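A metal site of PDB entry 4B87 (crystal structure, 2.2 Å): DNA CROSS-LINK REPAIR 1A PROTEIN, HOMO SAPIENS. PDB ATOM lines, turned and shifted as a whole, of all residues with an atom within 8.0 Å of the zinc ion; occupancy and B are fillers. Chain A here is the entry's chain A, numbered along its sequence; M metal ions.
OG1 of Thr 58 sits at hydrogen-bond distance from ND1 of His 59, at 2.9 Å. The backbone carbonyl oxygen of Glu 320 sits at hydrogen-bond distance from a ring nitrogen (ND1) of His 120 (2.9 Å). O of Ile 208 lies within hydrogen-bond range of NE2 of His 61 (2.9 Å).
The zinc ion is bound by a ring nitrogen (ND1) of His 61 (2.1 Å), the side-chain carboxylate of Asp 142 (2.1 Å), a ring nitrogen (NE2) of His 59 (2.1 Å) and a ring nitrogen (NE2) of His 120 (2.2 Å).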
ATOM      1  N   ASP A  42      21.675  -5.554  -2.729  1.00  0.00           N
ATOM      2  CA  ASP A  42      20.669  -4.461  -2.742  1.00  0.00           C
ATOM      3  C   ASP A  42      19.474  -4.834  -3.608  1.00  0.00           C
ATOM      4  O   ASP A  42      19.069  -4.057  -4.495  1.00  0.00           O
ATOM      5  CB  ASP A  42      21.302  -3.134  -3.211  1.00  0.00           C
ATOM      6  CG  ASP A  42      22.513  -2.750  -2.318  1.00  0.00           C
ATOM      7  OD1 ASP A  42      22.657  -3.341  -1.197  1.00  0.00           O
ATOM      8  OD2 ASP A  42      23.352  -1.900  -2.748  1.00  0.00           O
ATOM      9  N   THR A  58      24.355  -3.193   0.912  1.00  0.00           N
ATOM     10  CA  THR A  58      25.629  -2.444   1.025  1.00  0.00           C
ATOM     11  C   THR A  58      25.507  -1.270   1.978  1.00  0.00           C
ATOM     12  O   THR A  58      26.466  -0.955   2.741  1.00  0.00           O
ATOM     13  CB  THR A  58      26.154  -1.934  -0.313  1.00  0.00           C
ATOM     14  OG1 THR A  58      25.178  -1.054  -0.910  1.00  0.00           O
ATOM     15  CG2 THR A  58      26.448  -3.138  -1.318  1.00  0.00           C
ATOM     16  N   HIS A  59      24.351  -0.632   1.992  1.00  0.00           N
ATOM     17  CA  HIS A  59      24.164   0.530   2.876  1.00  0.00           C
ATOM     18  C   HIS A  59      22.711   0.996   2.989  1.00  0.00           C
ATOM     19  O   HIS A  59      21.865   0.670   2.123  1.00  0.00           O
ATOM     20  CB  HIS A  59      25.078   1.677   2.434  1.00  0.00           C
ATOM     21  CG  HIS A  59      24.711   2.355   1.138  1.00  0.00           C
ATOM     22  ND1 HIS A  59      24.725   1.728  -0.103  1.00  0.00           N
ATOM     23  CD2 HIS A  59      24.417   3.664   0.891  1.00  0.00           C
ATOM     24  CE1 HIS A  59      24.425   2.617  -1.058  1.00  0.00           C
ATOM     25  NE2 HIS A  59      24.255   3.798  -0.463  1.00  0.00           N
ATOM     26  N   PHE A  60      22.435   1.791   4.036  1.00  0.00           N
ATOM     27  CA  PHE A  60      21.045   2.158   4.347  1.00  0.00           C
ATOM     28  C   PHE A  60      20.655   3.434   3.559  1.00  0.00           C
ATOM     29  O   PHE A  60      20.439   4.477   4.161  1.00  0.00           O
ATOM     30  CB  PHE A  60      20.876   2.319   5.860  1.00  0.00           C
ATOM     31  CG  PHE A  60      19.446   2.376   6.310  1.00  0.00           C
ATOM     32  CD1 PHE A  60      18.650   1.207   6.363  1.00  0.00           C
ATOM     33  CD2 PHE A  60      18.854   3.627   6.656  1.00  0.00           C
ATOM     34  CE1 PHE A  60      17.307   1.270   6.785  1.00  0.00           C
ATOM     35  CE2 PHE A  60      17.503   3.690   7.089  1.00  0.00           C
ATOM     36  CZ  PHE A  60      16.740   2.511   7.157  1.00  0.00           C
ATOM     37  N   HIS A  61      20.637   3.362   2.210  1.00  0.00           N
ATOM     38  CA  HIS A  61      19.999   4.374   1.375  1.00  0.00           C
ATOM     39  C   HIS A  61      18.783   3.756   0.731  1.00  0.00           C
ATOM     40  O   HIS A  61      18.842   2.590   0.300  1.00  0.00           O
ATOM     41  CB  HIS A  61      20.973   4.923   0.294  1.00  0.00           C
ATOM     42  CG  HIS A  61      21.897   5.977   0.835  1.00  0.00           C
ATOM     43  ND1 HIS A  61      23.026   6.408   0.170  1.00  0.00           N
ATOM     44  CD2 HIS A  61      21.832   6.730   1.986  1.00  0.00           C
ATOM     45  CE1 HIS A  61      23.610   7.376   0.874  1.00  0.00           C
ATOM     46  NE2 HIS A  61      22.906   7.600   1.978  1.00  0.00           N
ATOM     47  N   SER A  62      17.713   4.520   0.578  1.00  0.00           N
ATOM     48  CA  SER A  62      16.430   3.902   0.335  1.00  0.00           C
ATOM     49  C   SER A  62      16.364   3.169  -1.026  1.00  0.00           C
ATOM     50  O   SER A  62      15.624   2.177  -1.158  1.00  0.00           O
ATOM     51  CB  SER A  62      15.286   4.943   0.516  1.00  0.00           C
ATOM     52  OG  SER A  62      15.376   5.889  -0.549  1.00  0.00           O
ATOM     53  N   ASP A  63      17.123   3.622  -2.029  1.00  0.00           N
ATOM     54  CA  ASP A  63      17.152   2.950  -3.341  1.00  0.00           C
ATOM     55  C   ASP A  63      17.691   1.516  -3.166  1.00  0.00           C
ATOM     56  O   ASP A  63      17.446   0.725  -4.009  1.00  0.00           O
ATOM     57  CB  ASP A  63      18.152   3.596  -4.311  1.00  0.00           C
ATOM     58  CG  ASP A  63      17.584   4.864  -5.012  1.00  0.00           C
ATOM     59  OD1 ASP A  63      16.352   5.035  -4.996  1.00  0.00           O
ATOM     60  OD2 ASP A  63      18.401   5.688  -5.548  1.00  0.00           O
ATOM     61  N   HIS A  64      18.508   1.273  -2.137  1.00  0.00           N
ATOM     62  CA  HIS A  64      19.175  -0.003  -1.924  1.00  0.00           C
ATOM     63  C   HIS A  64      18.364  -0.859  -0.979  1.00  0.00           C
ATOM     64  O   HIS A  64      18.141  -2.041  -1.231  1.00  0.00           O
ATOM     65  CB  HIS A  64      20.645   0.219  -1.500  1.00  0.00           C
ATOM     66  CG  HIS A  64      21.375   1.088  -2.451  1.00  0.00           C
ATOM     67  ND1 HIS A  64      22.358   0.619  -3.309  1.00  0.00           N
ATOM     68  CD2 HIS A  64      21.224   2.408  -2.747  1.00  0.00           C
ATOM     69  CE1 HIS A  64      22.757   1.592  -4.099  1.00  0.00           C
ATOM     70  NE2 HIS A  64      22.081   2.694  -3.779  1.00  0.00           N
ATOM     71  N   HIS A 120      31.427   6.114   2.047  1.00  0.00           N
ATOM     72  CA  HIS A 120      30.234   6.621   1.432  1.00  0.00           C
ATOM     73  C   HIS A 120      29.454   7.250   2.557  1.00  0.00           C
ATOM     74  O   HIS A 120      29.700   8.373   2.839  1.00  0.00           O
ATOM     75  CB  HIS A 120      29.447   5.480   0.727  1.00  0.00           C
ATOM     76  CG  HIS A 120      28.135   5.900   0.100  1.00  0.00           C
ATOM     77  ND1 HIS A 120      28.018   6.904  -0.836  1.00  0.00           N
ATOM     78  CD2 HIS A 120      26.893   5.378   0.252  1.00  0.00           C
ATOM     79  CE1 HIS A 120      26.739   7.010  -1.205  1.00  0.00           C
ATOM     80  NE2 HIS A 120      26.045   6.067  -0.583  1.00  0.00           N
ATOM     81  N   CYS A 121      28.568   6.549   3.232  1.00  0.00           N
ATOM     82  CA  CYS A 121      27.816   7.108   4.366  1.00  0.00           C
ATOM     83  C   CYS A 121      28.068   6.157   5.569  1.00  0.00           C
ATOM     84  O   CYS A 121      28.707   5.144   5.352  1.00  0.00           O
ATOM     85  CB  CYS A 121      26.334   7.153   4.020  1.00  0.00           C
ATOM     86  SG  CYS A 121      25.546   5.521   3.763  1.00  0.00           S
ATOM     87  N   ALA A 124      28.192   1.976   5.237  1.00  0.00           N
ATOM     88  CA  ALA A 124      28.320   1.575   3.838  1.00  0.00           C
ATOM     89  C   ALA A 124      29.584   0.700   3.654  1.00  0.00           C
ATOM     90  O   ALA A 124      30.689   1.042   4.163  1.00  0.00           O
ATOM     91  CB  ALA A 124      28.337   2.807   2.953  1.00  0.00           C
ATOM     92  N   GLY A 141      29.329  -1.402  -3.885  1.00  0.00           N
ATOM     93  CA  GLY A 141      28.110  -0.758  -3.400  1.00  0.00           C
ATOM     94  C   GLY A 141      28.173   0.710  -3.900  1.00  0.00           C
ATOM     95  O   GLY A 141      28.651   0.987  -4.990  1.00  0.00           O
ATOM     96  N   ASP A 142      27.786   1.666  -3.045  1.00  0.00           N
ATOM     97  CA  ASP A 142      28.105   3.076  -3.366  1.00  0.00           C
ATOM     98  C   ASP A 142      29.428   3.373  -2.663  1.00  0.00           C
ATOM     99  O   ASP A 142      29.622   3.013  -1.505  1.00  0.00           O
ATOM    100  CB  ASP A 142      27.071   4.048  -2.805  1.00  0.00           C
ATOM    101  CG  ASP A 142      25.820   4.179  -3.671  1.00  0.00           C
ATOM    102  OD1 ASP A 142      25.726   3.624  -4.803  1.00  0.00           O
ATOM    103  OD2 ASP A 142      24.879   4.851  -3.181  1.00  0.00           O
ATOM    104  N   PHE A 143      30.345   4.063  -3.334  1.00  0.00           N
ATOM    105  CA  PHE A 143      31.573   4.362  -2.653  1.00  0.00           C
ATOM    106  C   PHE A 143      32.114   5.699  -3.176  1.00  0.00           C
ATOM    107  O   PHE A 143      31.773   6.168  -4.281  1.00  0.00           O
ATOM    108  CB  PHE A 143      32.603   3.171  -2.751  1.00  0.00           C
ATOM    109  CG  PHE A 143      33.378   3.130  -4.064  1.00  0.00           C
ATOM    110  CD1 PHE A 143      32.755   3.332  -5.291  1.00  0.00           C
ATOM    111  CD2 PHE A 143      34.747   2.805  -4.066  1.00  0.00           C
ATOM    112  CE1 PHE A 143      33.469   3.248  -6.538  1.00  0.00           C
ATOM    113  CE2 PHE A 143      35.476   2.752  -5.298  1.00  0.00           C
ATOM    114  CZ  PHE A 143      34.835   2.985  -6.524  1.00  0.00           C
ATOM    115  N   ASP A 165      30.261   1.400  -8.718  1.00  0.00           N
ATOM    116  CA  ASP A 165      29.415   2.588  -8.564  1.00  0.00           C
ATOM    117  C   ASP A 165      29.825   3.655  -9.587  1.00  0.00           C
ATOM    118  O   ASP A 165      30.865   4.325  -9.453  1.00  0.00           O
ATOM    119  CB  ASP A 165      29.512   3.083  -7.133  1.00  0.00           C
ATOM    120  CG  ASP A 165      28.933   4.514  -6.933  1.00  0.00           C
ATOM    121  OD1 ASP A 165      28.163   4.998  -7.782  1.00  0.00           O
ATOM    122  OD2 ASP A 165      29.214   5.125  -5.902  1.00  0.00           O
ATOM    123  N   THR A 167      28.119   6.329 -10.498  1.00  0.00           N
ATOM    124  CA  THR A 167      27.253   7.497 -10.338  1.00  0.00           C
ATOM    125  C   THR A 167      27.787   8.663 -11.167  1.00  0.00           C
ATOM    126  O   THR A 167      27.037   9.275 -11.894  1.00  0.00           O
ATOM    127  CB  THR A 167      27.115   7.907  -8.835  1.00  0.00           C
ATOM    128  OG1 THR A 167      26.366   6.899  -8.158  1.00  0.00           O
ATOM    129  CG2 THR A 167      26.401   9.221  -8.664  1.00  0.00           C
ATOM    130  N   TYR A 206      17.843  14.112   3.767  1.00  0.00           N
ATOM    131  CA  TYR A 206      16.769  13.162   3.483  1.00  0.00           C
ATOM    132  C   TYR A 206      17.247  11.721   3.661  1.00  0.00           C
ATOM    133  O   TYR A 206      16.598  10.835   3.229  1.00  0.00           O
ATOM    134  CB  TYR A 206      16.180  13.349   2.066  1.00  0.00           C
ATOM    135  CG  TYR A 206      17.163  13.077   0.992  1.00  0.00           C
ATOM    136  CD1 TYR A 206      17.967  14.064   0.499  1.00  0.00           C
ATOM    137  CD2 TYR A 206      17.286  11.800   0.443  1.00  0.00           C
ATOM    138  CE1 TYR A 206      18.887  13.827  -0.534  1.00  0.00           C
ATOM    139  CE2 TYR A 206      18.212  11.554  -0.560  1.00  0.00           C
ATOM    140  CZ  TYR A 206      19.033  12.583  -1.028  1.00  0.00           C
ATOM    141  OH  TYR A 206      19.949  12.387  -2.042  1.00  0.00           O
ATOM    142  N   SER A 207      18.384  11.488   4.280  1.00  0.00           N
ATOM    143  CA  SER A 207      18.922  10.158   4.367  1.00  0.00           C
ATOM    144  C   SER A 207      20.131  10.282   5.267  1.00  0.00           C
ATOM    145  O   SER A 207      20.498  11.401   5.699  1.00  0.00           O
ATOM    146  CB  SER A 207      19.384   9.723   2.966  1.00  0.00           C
ATOM    147  OG  SER A 207      20.491  10.495   2.570  1.00  0.00           O
ATOM    148  N   ILE A 208      20.756   9.156   5.591  1.00  0.00           N
ATOM    149  CA  ILE A 208      21.983   9.252   6.376  1.00  0.00           C
ATOM    150  C   ILE A 208      23.093   9.643   5.411  1.00  0.00           C
ATOM    151  O   ILE A 208      22.975   9.472   4.158  1.00  0.00           O
ATOM    152  CB  ILE A 208      22.309   7.958   7.156  1.00  0.00           C
ATOM    153  CG1 ILE A 208      22.512   6.785   6.249  1.00  0.00           C
ATOM    154  CG2 ILE A 208      21.191   7.699   8.146  1.00  0.00           C
ATOM    155  CD1 ILE A 208      23.108   5.550   6.881  1.00  0.00           C
ATOM    156  N   GLU A 320      29.337  12.069  -1.704  1.00  0.00           N
ATOM    157  CA  GLU A 320      29.795  10.765  -1.142  1.00  0.00           C
ATOM    158  C   GLU A 320      30.052   9.679  -2.209  1.00  0.00           C
ATOM    159  O   GLU A 320      30.170   8.471  -1.903  1.00  0.00           O
ATOM    160  CB  GLU A 320      28.857  10.298  -0.002  1.00  0.00           C
ATOM    161  CG  GLU A 320      28.896  11.263   1.208  1.00  0.00           C
ATOM    162  CD  GLU A 320      27.994  10.898   2.396  1.00  0.00           C
ATOM    163  OE1 GLU A 320      26.861  10.342   2.121  1.00  0.00           O
ATOM    164  OE2 GLU A 320      28.405  11.195   3.604  1.00  0.00           O
ATOM    165  N   HIS A 321      30.161  10.120  -3.461  1.00  0.00           N
ATOM    166  CA  HIS A 321      30.534   9.257  -4.574  1.00  0.00           C
ATOM    167  C   HIS A 321      31.866   9.694  -5.188  1.00  0.00           C
ATOM    168  O   HIS A 321      32.263  10.878  -5.092  1.00  0.00           O
ATOM    169  CB  HIS A 321      29.468   9.265  -5.662  1.00  0.00           C
ATOM    170  CG  HIS A 321      28.131   8.819  -5.180  1.00  0.00           C
ATOM    171  ND1 HIS A 321      27.712   7.487  -5.242  1.00  0.00           N
ATOM    172  CD2 HIS A 321      27.108   9.522  -4.594  1.00  0.00           C
ATOM    173  CE1 HIS A 321      26.473   7.418  -4.771  1.00  0.00           C
ATOM    174  NE2 HIS A 321      26.096   8.635  -4.363  1.00  0.00           N
HETATM  175 ZN    ZN M   1      24.088   5.655  -1.421  1.00  0.00          ZN
